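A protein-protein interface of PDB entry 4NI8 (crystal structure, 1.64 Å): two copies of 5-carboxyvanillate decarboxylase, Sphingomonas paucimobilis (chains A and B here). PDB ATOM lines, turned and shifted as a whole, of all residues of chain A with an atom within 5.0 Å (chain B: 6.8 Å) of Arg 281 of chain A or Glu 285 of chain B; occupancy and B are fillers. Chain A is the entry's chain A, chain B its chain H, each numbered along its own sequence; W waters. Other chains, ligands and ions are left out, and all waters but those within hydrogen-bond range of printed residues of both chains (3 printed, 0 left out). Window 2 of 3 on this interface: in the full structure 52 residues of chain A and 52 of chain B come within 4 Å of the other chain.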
ATOM      1  N   HIS A 277      12.981  -7.938 -22.202  1.00  0.00           N
ATOM      2  CA  HIS A 277      12.962  -8.356 -23.602  1.00  0.00           C
ATOM      3  C   HIS A 277      13.910  -7.505 -24.442  1.00  0.00           C
ATOM      4  O   HIS A 277      14.528  -8.010 -25.376  1.00  0.00           O
ATOM      5  CB  HIS A 277      11.538  -8.289 -24.167  1.00  0.00           C
ATOM      6  CG  HIS A 277      10.635  -9.357 -23.635  1.00  0.00           C
ATOM      7  ND1 HIS A 277       9.260  -9.231 -23.616  1.00  0.00           N
ATOM      8  CD2 HIS A 277      10.910 -10.578 -23.119  1.00  0.00           C
ATOM      9  CE1 HIS A 277       8.729 -10.329 -23.105  1.00  0.00           C
ATOM     10  NE2 HIS A 277       9.707 -11.157 -22.786  1.00  0.00           N
ATOM     11  N   ALA A 278      14.028  -6.219 -24.110  1.00  0.00           N
ATOM     12  CA  ALA A 278      14.928  -5.331 -24.853  1.00  0.00           C
ATOM     13  C   ALA A 278      16.381  -5.742 -24.668  1.00  0.00           C
ATOM     14  O   ALA A 278      17.151  -5.741 -25.622  1.00  0.00           O
ATOM     15  CB  ALA A 278      14.745  -3.878 -24.412  1.00  0.00           C
ATOM     16  N   ALA A 279      16.762  -6.058 -23.433  1.00  0.00           N
ATOM     17  CA  ALA A 279      18.142  -6.454 -23.154  1.00  0.00           C
ATOM     18  C   ALA A 279      18.440  -7.815 -23.783  1.00  0.00           C
ATOM     19  O   ALA A 279      19.531  -8.034 -24.311  1.00  0.00           O
ATOM     20  CB  ALA A 279      18.404  -6.478 -21.643  1.00  0.00           C
ATOM     21  N   LEU A 280      17.457  -8.710 -23.737  1.00  0.00           N
ATOM     22  CA  LEU A 280      17.572 -10.022 -24.390  1.00  0.00           C
ATOM     23  C   LEU A 280      17.803  -9.891 -25.897  1.00  0.00           C
ATOM     24  O   LEU A 280      18.704 -10.515 -26.461  1.00  0.00           O
ATOM     25  CB  LEU A 280      16.323 -10.867 -24.120  1.00  0.00           C
ATOM     26  CG  LEU A 280      16.262 -12.206 -24.865  1.00  0.00           C
ATOM     27  CD1 LEU A 280      17.411 -13.121 -24.454  1.00  0.00           C
ATOM     28  CD2 LEU A 280      14.926 -12.866 -24.589  1.00  0.00           C
ATOM     29  N   ARG A 281      16.993  -9.060 -26.550  1.00  0.00           N
ATOM     30  CA  ARG A 281      17.127  -8.848 -27.994  1.00  0.00           C
ATOM     31  C   ARG A 281      18.474  -8.232 -28.348  1.00  0.00           C
ATOM     32  O   ARG A 281      19.110  -8.641 -29.326  1.00  0.00           O
ATOM     33  CB  ARG A 281      15.980  -7.990 -28.529  1.00  0.00           C
ATOM     34  CG  ARG A 281      14.693  -8.772 -28.779  1.00  0.00           C
ATOM     35  CD  ARG A 281      13.537  -7.830 -29.117  1.00  0.00           C
ATOM     36  NE  ARG A 281      13.933  -6.788 -30.065  1.00  0.00           N
ATOM     37  CZ  ARG A 281      14.015  -5.492 -29.769  1.00  0.00           C
ATOM     38  NH1 ARG A 281      14.384  -4.620 -30.697  1.00  0.00           N
ATOM     39  NH2 ARG A 281      13.721  -5.063 -28.548  1.00  0.00           N
ATOM     40  N   TYR A 282      18.900  -7.243 -27.557  1.00  0.00           N
ATOM     41  CA  TYR A 282      20.214  -6.639 -27.753  1.00  0.00           C
ATOM     42  C   TYR A 282      21.312  -7.714 -27.673  1.00  0.00           C
ATOM     43  O   TYR A 282      22.224  -7.746 -28.503  1.00  0.00           O
ATOM     44  CB  TYR A 282      20.483  -5.507 -26.739  1.00  0.00           C
ATOM     45  CG  TYR A 282      21.922  -5.058 -26.804  1.00  0.00           C
ATOM     46  CD1 TYR A 282      22.318  -4.062 -27.694  1.00  0.00           C
ATOM     47  CD2 TYR A 282      22.899  -5.670 -26.021  1.00  0.00           C
ATOM     48  CE1 TYR A 282      23.649  -3.685 -27.795  1.00  0.00           C
ATOM     49  CE2 TYR A 282      24.227  -5.304 -26.114  1.00  0.00           C
ATOM     50  CZ  TYR A 282      24.593  -4.305 -26.992  1.00  0.00           C
ATOM     51  OH  TYR A 282      25.918  -3.952 -27.088  1.00  0.00           O
ATOM     52  N   SER A 283      21.212  -8.593 -26.682  1.00  0.00           N
ATOM     53  CA  SER A 283      22.264  -9.578 -26.434  1.00  0.00           C
ATOM     54  C   SER A 283      22.322 -10.620 -27.546  1.00  0.00           C
ATOM     55  O   SER A 283      23.401 -11.011 -28.000  1.00  0.00           O
ATOM     56  CB  SER A 283      22.055 -10.242 -25.072  1.00  0.00           C
ATOM     57  OG  SER A 283      22.228  -9.261 -24.055  1.00  0.00           O
ATOM     58  N   ILE A 284      21.153 -11.068 -27.985  1.00  0.00           N
ATOM     59  CA  ILE A 284      21.078 -11.993 -29.112  1.00  0.00           C
ATOM     60  C   ILE A 284      21.663 -11.349 -30.363  1.00  0.00           C
ATOM     61  O   ILE A 284      22.389 -11.988 -31.123  1.00  0.00           O
ATOM     62  CB  ILE A 284      19.627 -12.424 -29.376  1.00  0.00           C
ATOM     63  CG1 ILE A 284      19.134 -13.301 -28.222  1.00  0.00           C
ATOM     64  CG2 ILE A 284      19.501 -13.167 -30.727  1.00  0.00           C
ATOM     65  CD1 ILE A 284      17.638 -13.541 -28.241  1.00  0.00           C
ATOM     66  N   GLU A 285      21.371 -10.068 -30.569  1.00  0.00           N
ATOM     67  CA  GLU A 285      21.924  -9.368 -31.726  1.00  0.00           C
ATOM     68  C   GLU A 285      23.461  -9.278 -31.747  1.00  0.00           C
ATOM     69  O   GLU A 285      24.090  -9.476 -32.801  1.00  0.00           O
ATOM     70  CB  GLU A 285      21.325  -7.957 -31.850  1.00  0.00           C
ATOM     71  CG  GLU A 285      21.974  -7.151 -32.957  1.00  0.00           C
ATOM     72  CD  GLU A 285      21.317  -5.803 -33.192  1.00  0.00           C
ATOM     73  OE1 GLU A 285      20.284  -5.511 -32.542  1.00  0.00           O
ATOM     74  OE2 GLU A 285      21.845  -5.030 -34.032  1.00  0.00           O
ATOM     75  N   PRO A 314       9.692 -11.811 -27.545  1.00  0.00           N
ATOM     76  CA  PRO A 314       9.334 -11.501 -28.935  1.00  0.00           C
ATOM     77  C   PRO A 314      10.469 -11.898 -29.888  1.00  0.00           C
ATOM     78  O   PRO A 314      11.083 -11.045 -30.542  1.00  0.00           O
ATOM     79  CB  PRO A 314       9.138  -9.981 -28.908  1.00  0.00           C
ATOM     80  CG  PRO A 314      10.054  -9.510 -27.819  1.00  0.00           C
ATOM     81  CD  PRO A 314      10.074 -10.611 -26.775  1.00  0.00           C
ATOM     82  N   ILE A 315      10.738 -13.202 -29.935  1.00  0.00           N
ATOM     83  CA  ILE A 315      11.762 -13.798 -30.791  1.00  0.00           C
ATOM     84  C   ILE A 315      11.165 -15.026 -31.481  1.00  0.00           C
ATOM     85  O   ILE A 315      10.196 -15.606 -30.988  1.00  0.00           O
ATOM     86  CB  ILE A 315      13.008 -14.199 -29.963  1.00  0.00           C
ATOM     87  CG1 ILE A 315      12.631 -15.153 -28.827  1.00  0.00           C
ATOM     88  CG2 ILE A 315      13.678 -12.941 -29.407  1.00  0.00           C
ATOM     89  CD1 ILE A 315      13.788 -15.506 -27.876  1.00  0.00           C
ATOM     90  N   LEU B 280      22.675   1.977 -29.477  1.00  0.00           N
ATOM     91  CA  LEU B 280      21.859   3.169 -29.703  1.00  0.00           C
ATOM     92  C   LEU B 280      20.380   2.802 -29.746  1.00  0.00           C
ATOM     93  O   LEU B 280      19.552   3.436 -29.086  1.00  0.00           O
ATOM     94  CB  LEU B 280      22.253   3.850 -31.016  1.00  0.00           C
ATOM     95  CG  LEU B 280      21.371   5.025 -31.472  1.00  0.00           C
ATOM     96  CD1 LEU B 280      21.395   6.172 -30.468  1.00  0.00           C
ATOM     97  CD2 LEU B 280      21.810   5.513 -32.851  1.00  0.00           C
ATOM     98  N   ARG B 281      20.042   1.765 -30.511  1.00  0.00           N
ATOM     99  CA  ARG B 281      18.638   1.370 -30.625  1.00  0.00           C
ATOM    100  C   ARG B 281      18.088   0.893 -29.293  1.00  0.00           C
ATOM    101  O   ARG B 281      16.968   1.249 -28.941  1.00  0.00           O
ATOM    102  CB  ARG B 281      18.433   0.303 -31.702  1.00  0.00           C
ATOM    103  CG  ARG B 281      18.477   0.863 -33.122  1.00  0.00           C
ATOM    104  CD  ARG B 281      18.044  -0.158 -34.166  1.00  0.00           C
ATOM    105  NE  ARG B 281      18.968  -1.287 -34.221  1.00  0.00           N
ATOM    106  CZ  ARG B 281      18.786  -2.438 -33.580  1.00  0.00           C
ATOM    107  NH1 ARG B 281      17.703  -2.632 -32.838  1.00  0.00           N
ATOM    108  NH2 ARG B 281      19.690  -3.395 -33.688  1.00  0.00           N
ATOM    109  N   TYR B 282      18.877   0.097 -28.566  1.00  0.00           N
ATOM    110  CA  TYR B 282      18.503  -0.347 -27.225  1.00  0.00           C
ATOM    111  C   TYR B 282      18.170   0.858 -26.339  1.00  0.00           C
ATOM    112  O   TYR B 282      17.166   0.871 -25.623  1.00  0.00           O
ATOM    113  CB  TYR B 282      19.628  -1.179 -26.560  1.00  0.00           C
ATOM    114  CG  TYR B 282      19.305  -1.449 -25.107  1.00  0.00           C
ATOM    115  CD1 TYR B 282      18.514  -2.536 -24.750  1.00  0.00           C
ATOM    116  CD2 TYR B 282      19.736  -0.585 -24.097  1.00  0.00           C
ATOM    117  CE1 TYR B 282      18.175  -2.768 -23.428  1.00  0.00           C
ATOM    118  CE2 TYR B 282      19.402  -0.816 -22.760  1.00  0.00           C
ATOM    119  CZ  TYR B 282      18.618  -1.903 -22.438  1.00  0.00           C
ATOM    120  OH  TYR B 282      18.258  -2.122 -21.120  1.00  0.00           O
ATOM    121  N   SER B 283      19.029   1.865 -26.386  1.00  0.00           N
ATOM    122  CA  SER B 283      18.890   2.999 -25.480  1.00  0.00           C
ATOM    123  C   SER B 283      17.653   3.826 -25.827  1.00  0.00           C
ATOM    124  O   SER B 283      16.913   4.250 -24.941  1.00  0.00           O
ATOM    125  CB  SER B 283      20.148   3.860 -25.499  1.00  0.00           C
ATOM    126  OG  SER B 283      21.263   3.123 -25.008  1.00  0.00           O
ATOM    127  N   ILE B 284      17.438   4.053 -27.117  1.00  0.00           N
ATOM    128  CA  ILE B 284      16.220   4.731 -27.552  1.00  0.00           C
ATOM    129  C   ILE B 284      14.975   3.960 -27.105  1.00  0.00           C
ATOM    130  O   ILE B 284      13.997   4.552 -26.629  1.00  0.00           O
ATOM    131  CB  ILE B 284      16.215   4.959 -29.068  1.00  0.00           C
ATOM    132  CG1 ILE B 284      17.335   5.931 -29.444  1.00  0.00           C
ATOM    133  CG2 ILE B 284      14.833   5.484 -29.534  1.00  0.00           C
ATOM    134  CD1 ILE B 284      17.549   6.030 -30.966  1.00  0.00           C
ATOM    135  N   GLU B 285      15.017   2.637 -27.219  1.00  0.00           N
ATOM    136  CA  GLU B 285      13.884   1.811 -26.801  1.00  0.00           C
ATOM    137  C   GLU B 285      13.524   1.930 -25.309  1.00  0.00           C
ATOM    138  O   GLU B 285      12.345   2.006 -24.962  1.00  0.00           O
ATOM    139  CB  GLU B 285      14.116   0.338 -27.186  1.00  0.00           C
ATOM    140  CG  GLU B 285      12.998  -0.603 -26.730  1.00  0.00           C
ATOM    141  CD  GLU B 285      13.213  -2.047 -27.176  1.00  0.00           C
ATOM    142  OE1 GLU B 285      14.175  -2.307 -27.937  1.00  0.00           O
ATOM    143  OE2 GLU B 285      12.415  -2.921 -26.757  1.00  0.00           O
ATOM    144  N   VAL B 286      14.531   1.933 -24.436  1.00  0.00           N
ATOM    145  CA  VAL B 286      14.279   1.863 -23.002  1.00  0.00           C
ATOM    146  C   VAL B 286      14.255   3.237 -22.338  1.00  0.00           C
ATOM    147  O   VAL B 286      13.641   3.395 -21.281  1.00  0.00           O
ATOM    148  CB  VAL B 286      15.260   0.907 -22.244  1.00  0.00           C
ATOM    149  CG1 VAL B 286      15.244  -0.500 -22.887  1.00  0.00           C
ATOM    150  CG2 VAL B 286      16.675   1.462 -22.209  1.00  0.00           C
ATOM    151  N   LEU B 287      14.881   4.232 -22.969  1.00  0.00           N
ATOM    152  CA  LEU B 287      14.902   5.586 -22.399  1.00  0.00           C
ATOM    153  C   LEU B 287      13.922   6.522 -23.087  1.00  0.00           C
ATOM    154  O   LEU B 287      13.465   7.502 -22.491  1.00  0.00           O
ATOM    155  CB  LEU B 287      16.301   6.204 -22.477  1.00  0.00           C
ATOM    156  CG  LEU B 287      17.423   5.391 -21.844  1.00  0.00           C
ATOM    157  CD1 LEU B 287      18.721   6.158 -21.961  1.00  0.00           C
ATOM    158  CD2 LEU B 287      17.096   5.113 -20.387  1.00  0.00           C
ATOM    159  N   GLY B 288      13.625   6.238 -24.350  1.00  0.00           N
ATOM    160  CA  GLY B 288      12.846   7.157 -25.163  1.00  0.00           C
ATOM    161  C   GLY B 288      13.785   7.989 -26.021  1.00  0.00           C
ATOM    162  O   GLY B 288      14.913   8.268 -25.609  1.00  0.00           O
ATOM    163  N   PRO B 289      13.331   8.388 -27.216  1.00  0.00           N
ATOM    164  CA  PRO B 289      14.236   9.092 -28.138  1.00  0.00           C
ATOM    165  C   PRO B 289      14.582  10.519 -27.690  1.00  0.00           C
ATOM    166  O   PRO B 289      15.555  11.082 -28.189  1.00  0.00           O
ATOM    167  CB  PRO B 289      13.453   9.103 -29.455  1.00  0.00           C
ATOM    168  CG  PRO B 289      12.016   9.020 -29.045  1.00  0.00           C
ATOM    169  CD  PRO B 289      12.010   8.128 -27.823  1.00  0.00           C
ATOM    170  N   VAL B 292      18.372  10.671 -25.642  1.00  0.00           N
ATOM    171  CA  VAL B 292      19.656  10.271 -26.210  1.00  0.00           C
ATOM    172  C   VAL B 292      20.225  11.352 -27.135  1.00  0.00           C
ATOM    173  O   VAL B 292      19.540  11.843 -28.040  1.00  0.00           O
ATOM    174  CB  VAL B 292      19.542   8.930 -27.003  1.00  0.00           C
ATOM    175  CG1 VAL B 292      20.914   8.474 -27.473  1.00  0.00           C
ATOM    176  CG2 VAL B 292      18.861   7.850 -26.158  1.00  0.00           C
HETATM  177  O   HOH W   1      21.463  -2.338 -34.998  1.00  0.00           O
HETATM  178  O   HOH W   2      11.530  -5.843 -26.855  1.00  0.00           O
HETATM  179  O   HOH W   3      17.019  -3.841 -27.908  1.00  0.00           O
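NH2 of Arg 281 of chain A is in salt-bridge range of OE1 of Glu 285 of chain B.
The guanidinium group (NH2) of Arg 281 of chain B is in salt-bridge range of the side-chain carboxylate (OE1) of Glu 285 of chain A, 2.5 Å away.
O of Ala 279 of chain A is in hydrogen-bond range of OG of Ser 283 of chain A.
Among the printed residues, merely in contact across the chains: Ala 278 of chain A with Tyr 282 of chain B, Ala 278 of chain A with Glu 285 of chain B, Ala 278 of chain A with Val 286 of chain B and Ala 279 of chain A with Tyr 282 of chain B.
Of the printed residues of chain B, Ala 279 of chain A touches Tyr 282 (3.6 Å).
Of chain B, only Glu 285 comes within 4 Å of Arg 281 of chain A.
Of the printed residues of chain B, Glu 285 of chain A touches Arg 281 (2.5 Å).
Printed residues of chain A within 4 Å of Tyr 282 of chain B: Ala 278 (3.6 Å) and Ala 279 (3.6 Å).
Glu 285 of chain B touches just these residues of chain A: Ala 278 (3.4 Å) and Arg 281 (2.9 Å).
The nearest printed residue of chain A that does not touch Glu 285 of chain B is His 277 of chain A (5.3 Å).
Printed residues of chain A that touch a printed residue of chain B: Ala 278, Ala 279, Arg 281 and Glu 285.
Hydrophobic or aromatic side chains of chain A within 4 Å of the printed part of chain B: Ala 278.
Among the printed residues, 6 pairs touch across the chains.
Among the printed residues, Asp or Glu carboxylates within 4 Å of a Lys or Arg side-chain nitrogen of the other chain: Arg 281 of chain A with Glu 285 of chain B (2.9 Å) and Glu 285 of chain A with Arg 281 of chain B (2.5 Å).
Arg 281 of chain A touches Glu 285 of chain B, and with the chains exchanged Glu 285 of chain A touches Arg 281 of chain B.
6 positions are printed for both chains.
Water W1 bridges the guanidinium group of Arg 281 of chain B (2.4 Å) and the side-chain carboxylate of Glu 285 of chain A (2.9 Å).
Water W2 lies within hydrogen-bond range of the guanidinium group (NH2) of Arg 281 of chain A (2.9 Å) and the side-chain carboxylate (OE2) of Glu 285 of chain B (3.1 Å).
Water W3 lies within hydrogen-bond range of the backbone carbonyl oxygen (O) of Ala 278 of chain A and the side-chain carboxylate (OE1) of Glu 285 of chain B.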
